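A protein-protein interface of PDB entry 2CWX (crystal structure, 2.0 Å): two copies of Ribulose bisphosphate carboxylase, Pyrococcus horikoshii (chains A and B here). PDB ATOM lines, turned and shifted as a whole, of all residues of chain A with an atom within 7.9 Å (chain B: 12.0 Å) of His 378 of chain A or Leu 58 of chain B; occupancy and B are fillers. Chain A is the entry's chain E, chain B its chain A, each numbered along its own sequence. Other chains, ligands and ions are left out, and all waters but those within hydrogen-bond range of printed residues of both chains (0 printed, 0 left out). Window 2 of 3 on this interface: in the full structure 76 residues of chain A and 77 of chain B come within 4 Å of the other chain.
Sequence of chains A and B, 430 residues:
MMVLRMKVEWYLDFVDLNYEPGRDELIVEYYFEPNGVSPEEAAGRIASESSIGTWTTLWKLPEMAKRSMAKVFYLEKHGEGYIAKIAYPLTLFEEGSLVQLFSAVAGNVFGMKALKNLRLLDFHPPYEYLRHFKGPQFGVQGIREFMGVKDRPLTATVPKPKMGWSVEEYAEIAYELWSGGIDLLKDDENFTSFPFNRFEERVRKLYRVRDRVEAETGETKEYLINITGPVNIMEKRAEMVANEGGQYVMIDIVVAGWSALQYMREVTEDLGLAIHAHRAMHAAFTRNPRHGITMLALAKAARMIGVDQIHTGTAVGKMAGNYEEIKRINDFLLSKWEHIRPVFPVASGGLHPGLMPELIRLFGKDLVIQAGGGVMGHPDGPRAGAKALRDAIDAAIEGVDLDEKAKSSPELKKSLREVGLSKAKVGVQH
N of Asp 380 of chain A lies within hydrogen-bond range of ND1 of His 378 of chain A (3.1 Å).
The backbone carbonyl oxygen (O) of Glu 411 of chain A sits at hydrogen-bond distance from a ring nitrogen (NE2) of His 378 of chain A.
No position is printed for both chains.
Of the 4 pairs that touch across the chains among the printed residues, none has its exchanged pair printed and touching as well.
Of chain B, only Leu 58 comes within 4 Å of Met 376 of chain A.
His 378 of chain A touches one residue of chain B.
No residue of chain B comes within 4 Å of Pro 379 of chain A.
No residue of chain B comes within 4 Å of Asp 380 of chain A.
No residue of chain B comes within 4 Å of Gly 381 of chain A.
No residue of chain B comes within 4 Å of Ala 388 of chain A.
No residue of chain B comes within 4 Å of Glu 411 of chain A.
No residue of chain B comes within 4 Å of Ser 415 of chain A.
Of chain A, only Met 376, Gly 377 and His 378 come within 4 Å of Leu 58 of chain B.
Of the printed residues of chain A, Trp 59 of chain B touches Pro 382.
The nearest residue of chain A that does not touch Leu 58 of chain B is Pro 379 of chain A (4.4 Å).
The nearest printed residue of chain A that does not touch Trp 59 of chain B is Met 376 of chain A (4.7 Å).
Of the 7 printed residues of chain B, 2 touch a printed residue of chain A.
Hydrophobic or aromatic side chains of chain B within 4 Å of the printed part of chain A: Leu 58 and Trp 59.
Of the 27 printed residues of chain A, 4 touch a printed residue of chain B.
Printed residues of chain A that touch a printed residue of chain B: Met 376, Gly 377, His 378 and Pro 382.
Hydrophobic or aromatic side chains of chain A within 4 Å of the printed part of chain B: Pro 382.
Among the printed residues, 4 pairs touch across the chains.
Among the printed residues, no Asp or Glu carboxylate lies within 4 Å of a Lys or Arg side-chain nitrogen of the other chain.
Met 376 of chain A touches Leu 58 of chain B (O to CD2, 3.2 Å).
Leu 58 of chain B touches Gly 377 of chain A.
O of His 378 of chain A touches CD2 of Leu 58 of chain B (3.1 Å).
CE3 of Trp 59 of chain B touches CG of Pro 382 of chain A (3.5 Å).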
ATOM      1  N   PRO A 353      12.387   8.512  -3.148  1.00  0.00           N
ATOM      2  CA  PRO A 353      12.238   9.863  -2.600  1.00  0.00           C
ATOM      3  C   PRO A 353      13.539  10.568  -2.206  1.00  0.00           C
ATOM      4  O   PRO A 353      13.666  11.765  -2.477  1.00  0.00           O
ATOM      5  CB  PRO A 353      11.306   9.640  -1.410  1.00  0.00           C
ATOM      6  CG  PRO A 353      10.456   8.528  -1.858  1.00  0.00           C
ATOM      7  CD  PRO A 353      11.396   7.595  -2.553  1.00  0.00           C
ATOM      8  N   GLY A 372       9.165   3.736  -9.863  1.00  0.00           N
ATOM      9  CA  GLY A 372       8.367   2.570  -9.518  1.00  0.00           C
ATOM     10  C   GLY A 372       8.884   1.726  -8.360  1.00  0.00           C
ATOM     11  O   GLY A 372       8.104   1.275  -7.527  1.00  0.00           O
ATOM     12  N   GLY A 373      10.196   1.512  -8.321  1.00  0.00           N
ATOM     13  CA  GLY A 373      10.835   0.740  -7.262  1.00  0.00           C
ATOM     14  C   GLY A 373      10.582   1.321  -5.890  1.00  0.00           C
ATOM     15  O   GLY A 373      10.067   0.631  -4.990  1.00  0.00           O
ATOM     16  N   GLY A 374      10.935   2.600  -5.735  1.00  0.00           N
ATOM     17  CA  GLY A 374      10.782   3.306  -4.480  1.00  0.00           C
ATOM     18  C   GLY A 374       9.342   3.330  -4.011  1.00  0.00           C
ATOM     19  O   GLY A 374       9.065   3.159  -2.821  1.00  0.00           O
ATOM     20  N   VAL A 375       8.414   3.514  -4.944  1.00  0.00           N
ATOM     21  CA  VAL A 375       7.008   3.623  -4.600  1.00  0.00           C
ATOM     22  C   VAL A 375       6.416   2.267  -4.191  1.00  0.00           C
ATOM     23  O   VAL A 375       5.820   2.151  -3.128  1.00  0.00           O
ATOM     24  CB  VAL A 375       6.204   4.242  -5.755  1.00  0.00           C
ATOM     25  CG1 VAL A 375       4.727   4.119  -5.501  1.00  0.00           C
ATOM     26  CG2 VAL A 375       6.590   5.703  -5.931  1.00  0.00           C
ATOM     27  N   MET A 376       6.580   1.250  -5.030  1.00  0.00           N
ATOM     28  CA  MET A 376       5.948  -0.058  -4.815  1.00  0.00           C
ATOM     29  C   MET A 376       6.532  -0.774  -3.611  1.00  0.00           C
ATOM     30  O   MET A 376       5.809  -1.433  -2.882  1.00  0.00           O
ATOM     31  CB  MET A 376       6.124  -0.950  -6.047  1.00  0.00           C
ATOM     32  CG  MET A 376       5.344  -0.504  -7.267  1.00  0.00           C
ATOM     33  SD  MET A 376       3.544  -0.682  -7.105  1.00  0.00           S
ATOM     34  CE  MET A 376       3.371  -2.351  -6.506  1.00  0.00           C
ATOM     35  N   GLY A 377       7.842  -0.611  -3.423  1.00  0.00           N
ATOM     36  CA  GLY A 377       8.600  -1.210  -2.337  1.00  0.00           C
ATOM     37  C   GLY A 377       8.610  -0.473  -0.988  1.00  0.00           C
ATOM     38  O   GLY A 377       9.467  -0.739  -0.124  1.00  0.00           O
ATOM     39  N   HIS A 378       7.649   0.426  -0.792  1.00  0.00           N
ATOM     40  CA  HIS A 378       7.540   1.185   0.448  1.00  0.00           C
ATOM     41  C   HIS A 378       6.909   0.311   1.517  1.00  0.00           C
ATOM     42  O   HIS A 378       5.865  -0.287   1.283  1.00  0.00           O
ATOM     43  CB  HIS A 378       6.665   2.420   0.227  1.00  0.00           C
ATOM     44  CG  HIS A 378       6.669   3.372   1.374  1.00  0.00           C
ATOM     45  ND1 HIS A 378       5.787   3.268   2.430  1.00  0.00           N
ATOM     46  CD2 HIS A 378       7.467   4.431   1.652  1.00  0.00           C
ATOM     47  CE1 HIS A 378       6.027   4.235   3.299  1.00  0.00           C
ATOM     48  NE2 HIS A 378       7.039   4.956   2.849  1.00  0.00           N
ATOM     49  N   PRO A 379       7.494   0.289   2.712  1.00  0.00           N
ATOM     50  CA  PRO A 379       7.014  -0.615   3.773  1.00  0.00           C
ATOM     51  C   PRO A 379       5.541  -0.431   4.168  1.00  0.00           C
ATOM     52  O   PRO A 379       5.011  -1.342   4.767  1.00  0.00           O
ATOM     53  CB  PRO A 379       7.936  -0.297   4.953  1.00  0.00           C
ATOM     54  CG  PRO A 379       8.507   1.071   4.651  1.00  0.00           C
ATOM     55  CD  PRO A 379       8.626   1.127   3.161  1.00  0.00           C
ATOM     56  N   ASP A 380       4.905   0.696   3.851  1.00  0.00           N
ATOM     57  CA  ASP A 380       3.483   0.878   4.137  1.00  0.00           C
ATOM     58  C   ASP A 380       2.570   0.711   2.931  1.00  0.00           C
ATOM     59  O   ASP A 380       1.358   0.849   3.050  1.00  0.00           O
ATOM     60  CB  ASP A 380       3.252   2.227   4.791  1.00  0.00           C
ATOM     61  CG  ASP A 380       3.663   2.230   6.242  1.00  0.00           C
ATOM     62  OD1 ASP A 380       3.558   3.298   6.872  1.00  0.00           O
ATOM     63  OD2 ASP A 380       4.079   1.207   6.846  1.00  0.00           O
ATOM     64  N   GLY A 381       3.148   0.423   1.770  1.00  0.00           N
ATOM     65  CA  GLY A 381       2.382   0.124   0.577  1.00  0.00           C
ATOM     66  C   GLY A 381       2.571   1.157  -0.513  1.00  0.00           C
ATOM     67  O   GLY A 381       3.150   2.214  -0.287  1.00  0.00           O
ATOM     68  N   PRO A 382       2.056   0.854  -1.701  1.00  0.00           N
ATOM     69  CA  PRO A 382       2.191   1.753  -2.862  1.00  0.00           C
ATOM     70  C   PRO A 382       1.588   3.149  -2.627  1.00  0.00           C
ATOM     71  O   PRO A 382       2.171   4.124  -3.076  1.00  0.00           O
ATOM     72  CB  PRO A 382       1.421   1.040  -3.980  1.00  0.00           C
ATOM     73  CG  PRO A 382       0.831  -0.209  -3.388  1.00  0.00           C
ATOM     74  CD  PRO A 382       1.287  -0.371  -1.990  1.00  0.00           C
ATOM     75  N   ARG A 383       0.437   3.233  -1.959  1.00  0.00           N
ATOM     76  CA  ARG A 383      -0.206   4.523  -1.743  1.00  0.00           C
ATOM     77  C   ARG A 383       0.727   5.434  -0.930  1.00  0.00           C
ATOM     78  O   ARG A 383       0.948   6.588  -1.278  1.00  0.00           O
ATOM     79  CB  ARG A 383      -1.549   4.347  -1.037  1.00  0.00           C
ATOM     80  CG  ARG A 383      -2.278   5.615  -0.765  1.00  0.00           C
ATOM     81  CD  ARG A 383      -3.671   5.397  -0.217  1.00  0.00           C
ATOM     82  NE  ARG A 383      -4.330   6.699  -0.086  1.00  0.00           N
ATOM     83  CZ  ARG A 383      -5.633   6.929  -0.263  1.00  0.00           C
ATOM     84  NH1 ARG A 383      -6.468   5.923  -0.534  1.00  0.00           N
ATOM     85  NH2 ARG A 383      -6.095   8.178  -0.155  1.00  0.00           N
ATOM     86  N   ALA A 384       1.309   4.865   0.119  1.00  0.00           N
ATOM     87  CA  ALA A 384       2.273   5.563   0.956  1.00  0.00           C
ATOM     88  C   ALA A 384       3.548   5.933   0.196  1.00  0.00           C
ATOM     89  O   ALA A 384       4.126   6.987   0.426  1.00  0.00           O
ATOM     90  CB  ALA A 384       2.609   4.699   2.210  1.00  0.00           C
ATOM     91  N   GLY A 385       3.985   5.068  -0.712  1.00  0.00           N
ATOM     92  CA  GLY A 385       5.186   5.312  -1.488  1.00  0.00           C
ATOM     93  C   GLY A 385       4.972   6.488  -2.424  1.00  0.00           C
ATOM     94  O   GLY A 385       5.853   7.331  -2.584  1.00  0.00           O
ATOM     95  N   ALA A 386       3.787   6.562  -3.019  1.00  0.00           N
ATOM     96  CA  ALA A 386       3.444   7.680  -3.893  1.00  0.00           C
ATOM     97  C   ALA A 386       3.468   8.985  -3.124  1.00  0.00           C
ATOM     98  O   ALA A 386       3.972   9.988  -3.601  1.00  0.00           O
ATOM     99  CB  ALA A 386       2.100   7.476  -4.499  1.00  0.00           C
ATOM    100  N   LYS A 387       2.901   8.949  -1.926  1.00  0.00           N
ATOM    101  CA  LYS A 387       2.834  10.114  -1.069  1.00  0.00           C
ATOM    102  C   LYS A 387       4.228  10.570  -0.739  1.00  0.00           C
ATOM    103  O   LYS A 387       4.540  11.744  -0.859  1.00  0.00           O
ATOM    104  CB  LYS A 387       2.078   9.776   0.216  1.00  0.00           C
ATOM    105  CG  LYS A 387       0.932  10.727   0.509  1.00  0.00           C
ATOM    106  CD  LYS A 387       1.415  12.004   1.148  1.00  0.00           C
ATOM    107  CE  LYS A 387       0.570  12.313   2.403  1.00  0.00           C
ATOM    108  NZ  LYS A 387       0.789  13.717   2.896  1.00  0.00           N
ATOM    109  N   ALA A 388       5.068   9.621  -0.362  1.00  0.00           N
ATOM    110  CA  ALA A 388       6.448   9.897  -0.015  1.00  0.00           C
ATOM    111  C   ALA A 388       7.190  10.588  -1.168  1.00  0.00           C
ATOM    112  O   ALA A 388       7.791  11.653  -0.973  1.00  0.00           O
ATOM    113  CB  ALA A 388       7.160   8.619   0.386  1.00  0.00           C
ATOM    114  N   LEU A 389       7.128   9.995  -2.355  1.00  0.00           N
ATOM    115  CA  LEU A 389       7.704  10.612  -3.545  1.00  0.00           C
ATOM    116  C   LEU A 389       7.195  12.050  -3.775  1.00  0.00           C
ATOM    117  O   LEU A 389       7.982  12.930  -4.024  1.00  0.00           O
ATOM    118  CB  LEU A 389       7.432   9.759  -4.800  1.00  0.00           C
ATOM    119  CG  LEU A 389       8.106  10.210  -6.101  1.00  0.00           C
ATOM    120  CD1 LEU A 389       9.605  10.019  -6.092  1.00  0.00           C
ATOM    121  CD2 LEU A 389       7.514   9.441  -7.258  1.00  0.00           C
ATOM    122  N   SER A 409       5.732  14.447   7.476  1.00  0.00           N
ATOM    123  CA  SER A 409       5.341  13.457   6.474  1.00  0.00           C
ATOM    124  C   SER A 409       5.775  12.061   6.915  1.00  0.00           C
ATOM    125  O   SER A 409       6.896  11.645   6.633  1.00  0.00           O
ATOM    126  CB  SER A 409       5.944  13.795   5.095  1.00  0.00           C
ATOM    127  OG  SER A 409       5.572  12.807   4.115  1.00  0.00           O
ATOM    128  N   PRO A 410       4.896  11.351   7.633  1.00  0.00           N
ATOM    129  CA  PRO A 410       5.216   9.999   8.113  1.00  0.00           C
ATOM    130  C   PRO A 410       5.642   9.066   6.984  1.00  0.00           C
ATOM    131  O   PRO A 410       6.556   8.270   7.160  1.00  0.00           O
ATOM    132  CB  PRO A 410       3.900   9.522   8.766  1.00  0.00           C
ATOM    133  CG  PRO A 410       3.161  10.766   9.118  1.00  0.00           C
ATOM    134  CD  PRO A 410       3.549  11.782   8.056  1.00  0.00           C
ATOM    135  N   GLU A 411       4.997   9.201   5.830  1.00  0.00           N
ATOM    136  CA  GLU A 411       5.280   8.372   4.655  1.00  0.00           C
ATOM    137  C   GLU A 411       6.726   8.607   4.165  1.00  0.00           C
ATOM    138  O   GLU A 411       7.508   7.672   4.003  1.00  0.00           O
ATOM    139  CB  GLU A 411       4.248   8.660   3.540  1.00  0.00           C
ATOM    140  CG  GLU A 411       2.780   8.321   3.881  1.00  0.00           C
ATOM    141  CD  GLU A 411       1.989   9.436   4.597  1.00  0.00           C
ATOM    142  OE1 GLU A 411       0.784   9.221   4.881  1.00  0.00           O
ATOM    143  OE2 GLU A 411       2.537  10.531   4.904  1.00  0.00           O
ATOM    144  N   LEU A 412       7.097   9.863   3.962  1.00  0.00           N
ATOM    145  CA  LEU A 412       8.480  10.163   3.589  1.00  0.00           C
ATOM    146  C   LEU A 412       9.484   9.719   4.657  1.00  0.00           C
ATOM    147  O   LEU A 412      10.556   9.216   4.327  1.00  0.00           O
ATOM    148  CB  LEU A 412       8.658  11.651   3.300  1.00  0.00           C
ATOM    149  CG  LEU A 412      10.068  12.052   2.879  1.00  0.00           C
ATOM    150  CD1 LEU A 412      10.431  11.384   1.575  1.00  0.00           C
ATOM    151  CD2 LEU A 412      10.184  13.581   2.788  1.00  0.00           C
ATOM    152  N   LYS A 413       9.138   9.909   5.931  1.00  0.00           N
ATOM    153  CA  LYS A 413      10.034   9.546   7.030  1.00  0.00           C
ATOM    154  C   LYS A 413      10.448   8.086   6.887  1.00  0.00           C
ATOM    155  O   LYS A 413      11.636   7.767   6.876  1.00  0.00           O
ATOM    156  CB  LYS A 413       9.356   9.785   8.383  1.00  0.00           C
ATOM    157  CG  LYS A 413      10.309   9.716   9.607  1.00  0.00           C
ATOM    158  CD  LYS A 413       9.611  10.109  10.895  1.00  0.00           C
ATOM    159  CE  LYS A 413      10.609  10.423  11.994  1.00  0.00           C
ATOM    160  NZ  LYS A 413       9.919  10.760  13.266  1.00  0.00           N
ATOM    161  N   LYS A 414       9.451   7.218   6.717  1.00  0.00           N
ATOM    162  CA  LYS A 414       9.672   5.778   6.609  1.00  0.00           C
ATOM    163  C   LYS A 414      10.498   5.414   5.373  1.00  0.00           C
ATOM    164  O   LYS A 414      11.317   4.500   5.419  1.00  0.00           O
ATOM    165  CB  LYS A 414       8.328   5.037   6.617  1.00  0.00           C
ATOM    166  CG  LYS A 414       7.530   5.207   7.932  1.00  0.00           C
ATOM    167  CD  LYS A 414       6.014   5.033   7.742  1.00  0.00           C
ATOM    168  CE  LYS A 414       5.281   4.849   9.099  1.00  0.00           C
ATOM    169  NZ  LYS A 414       4.783   3.442   9.339  1.00  0.00           N
ATOM    170  N   SER A 415      10.302   6.144   4.275  1.00  0.00           N
ATOM    171  CA  SER A 415      11.047   5.892   3.044  1.00  0.00           C
ATOM    172  C   SER A 415      12.549   6.185   3.198  1.00  0.00           C
ATOM    173  O   SER A 415      13.388   5.436   2.703  1.00  0.00           O
ATOM    174  CB  SER A 415      10.468   6.716   1.884  1.00  0.00           C
ATOM    175  OG  SER A 415      11.310   6.657   0.742  1.00  0.00           O
ATOM    176  N   LEU A 416      12.875   7.277   3.878  1.00  0.00           N
ATOM    177  CA  LEU A 416      14.271   7.688   4.080  1.00  0.00           C
ATOM    178  C   LEU A 416      15.052   6.712   4.984  1.00  0.00           C
ATOM    179  O   LEU A 416      16.277   6.612   4.883  1.00  0.00           O
ATOM    180  CB  LEU A 416      14.325   9.106   4.647  1.00  0.00           C
ATOM    181  CG  LEU A 416      13.645  10.177   3.780  1.00  0.00           C
ATOM    182  CD1 LEU A 416      13.305  11.416   4.623  1.00  0.00           C
ATOM    183  CD2 LEU A 416      14.518  10.542   2.576  1.00  0.00           C
ATOM    184  N   TRP B  10      16.820 -13.197  -5.377  1.00  0.00           N
ATOM    185  CA  TRP B  10      15.695 -13.136  -6.305  1.00  0.00           C
ATOM    186  C   TRP B  10      16.123 -13.459  -7.743  1.00  0.00           C
ATOM    187  O   TRP B  10      15.505 -14.283  -8.391  1.00  0.00           O
ATOM    188  CB  TRP B  10      15.026 -11.763  -6.239  1.00  0.00           C
ATOM    189  CG  TRP B  10      13.940 -11.575  -7.243  1.00  0.00           C
ATOM    190  CD1 TRP B  10      13.992 -10.788  -8.362  1.00  0.00           C
ATOM    191  CD2 TRP B  10      12.631 -12.169  -7.233  1.00  0.00           C
ATOM    192  NE1 TRP B  10      12.803 -10.857  -9.049  1.00  0.00           N
ATOM    193  CE2 TRP B  10      11.946 -11.695  -8.380  1.00  0.00           C
ATOM    194  CE3 TRP B  10      11.965 -13.059  -6.377  1.00  0.00           C
ATOM    195  CZ2 TRP B  10      10.635 -12.077  -8.684  1.00  0.00           C
ATOM    196  CZ3 TRP B  10      10.668 -13.441  -6.684  1.00  0.00           C
ATOM    197  CH2 TRP B  10      10.018 -12.950  -7.826  1.00  0.00           C
ATOM    198  N   THR B  54      10.924  -7.852 -10.855  1.00  0.00           N
ATOM    199  CA  THR B  54      11.235  -8.091  -9.437  1.00  0.00           C
ATOM    200  C   THR B  54      10.007  -7.987  -8.550  1.00  0.00           C
ATOM    201  O   THR B  54       8.897  -7.775  -9.052  1.00  0.00           O
ATOM    202  CB  THR B  54      12.240  -7.060  -8.958  1.00  0.00           C
ATOM    203  OG1 THR B  54      11.720  -5.752  -9.231  1.00  0.00           O
ATOM    204  CG2 THR B  54      13.535  -7.118  -9.772  1.00  0.00           C
ATOM    205  N   LEU B  58       5.120  -7.361   0.147  1.00  0.00           N
ATOM    206  CA  LEU B  58       4.363  -6.122   0.300  1.00  0.00           C
ATOM    207  C   LEU B  58       2.961  -6.257  -0.309  1.00  0.00           C
ATOM    208  O   LEU B  58       1.972  -6.413   0.414  1.00  0.00           O
ATOM    209  CB  LEU B  58       5.121  -4.963  -0.347  1.00  0.00           C
ATOM    210  CG  LEU B  58       6.070  -4.176   0.555  1.00  0.00           C
ATOM    211  CD1 LEU B  58       7.301  -4.979   0.971  1.00  0.00           C
ATOM    212  CD2 LEU B  58       6.490  -2.924  -0.164  1.00  0.00           C
ATOM    213  N   TRP B  59       2.886  -6.179  -1.637  1.00  0.00           N
ATOM    214  CA  TRP B  59       1.639  -6.400  -2.368  1.00  0.00           C
ATOM    215  C   TRP B  59       1.665  -7.810  -2.969  1.00  0.00           C
ATOM    216  O   TRP B  59       2.730  -8.318  -3.342  1.00  0.00           O
ATOM    217  CB  TRP B  59       1.449  -5.331  -3.453  1.00  0.00           C
ATOM    218  CG  TRP B  59       0.023  -5.185  -3.887  1.00  0.00           C
ATOM    219  CD1 TRP B  59      -0.645  -5.968  -4.786  1.00  0.00           C
ATOM    220  CD2 TRP B  59      -0.921  -4.215  -3.425  1.00  0.00           C
ATOM    221  NE1 TRP B  59      -1.946  -5.543  -4.916  1.00  0.00           N
ATOM    222  CE2 TRP B  59      -2.144  -4.466  -4.093  1.00  0.00           C
ATOM    223  CE3 TRP B  59      -0.865  -3.160  -2.506  1.00  0.00           C
ATOM    224  CZ2 TRP B  59      -3.291  -3.700  -3.876  1.00  0.00           C
ATOM    225  CZ3 TRP B  59      -2.002  -2.398  -2.293  1.00  0.00           C
ATOM    226  CH2 TRP B  59      -3.201  -2.671  -2.978  1.00  0.00           C
ATOM    227  N   LYS B  60       0.488  -8.431  -3.057  1.00  0.00           N
ATOM    228  CA  LYS B  60       0.364  -9.860  -3.401  1.00  0.00           C
ATOM    229  C   LYS B  60       0.915 -10.239  -4.797  1.00  0.00           C
ATOM    230  O   LYS B  60       0.294  -9.938  -5.819  1.00  0.00           O
ATOM    231  CB  LYS B  60      -1.107 -10.304  -3.261  1.00  0.00           C
ATOM    232  CG  LYS B  60      -1.307 -11.809  -3.019  1.00  0.00           C
ATOM    233  CD  LYS B  60      -2.720 -12.275  -3.417  1.00  0.00           C
ATOM    234  CE  LYS B  60      -2.925 -12.265  -4.929  1.00  0.00           C
ATOM    235  NZ  LYS B  60      -3.817 -11.148  -5.369  1.00  0.00           N
ATOM    236  N   LEU B  61       2.078 -10.906  -4.813  1.00  0.00           N
ATOM    237  CA  LEU B  61       2.741 -11.396  -6.043  1.00  0.00           C
ATOM    238  C   LEU B  61       1.798 -12.325  -6.842  1.00  0.00           C
ATOM    239  O   LEU B  61       1.622 -13.486  -6.443  1.00  0.00           O
ATOM    240  CB  LEU B  61       4.023 -12.144  -5.648  1.00  0.00           C
ATOM    241  CG  LEU B  61       4.962 -12.809  -6.672  1.00  0.00           C
ATOM    242  CD1 LEU B  61       4.494 -14.210  -7.076  1.00  0.00           C
ATOM    243  CD2 LEU B  61       5.212 -11.935  -7.900  1.00  0.00           C
ATOM    244  N   PRO B  62       1.205 -11.843  -7.951  1.00  0.00           N
ATOM    245  CA  PRO B  62       0.094 -12.568  -8.595  1.00  0.00           C
ATOM    246  C   PRO B  62       0.474 -13.980  -9.034  1.00  0.00           C
ATOM    247  O   PRO B  62       1.636 -14.224  -9.349  1.00  0.00           O
ATOM    248  CB  PRO B  62      -0.278 -11.697  -9.798  1.00  0.00           C
ATOM    249  CG  PRO B  62       0.449 -10.393  -9.640  1.00  0.00           C
ATOM    250  CD  PRO B  62       1.570 -10.619  -8.692  1.00  0.00           C
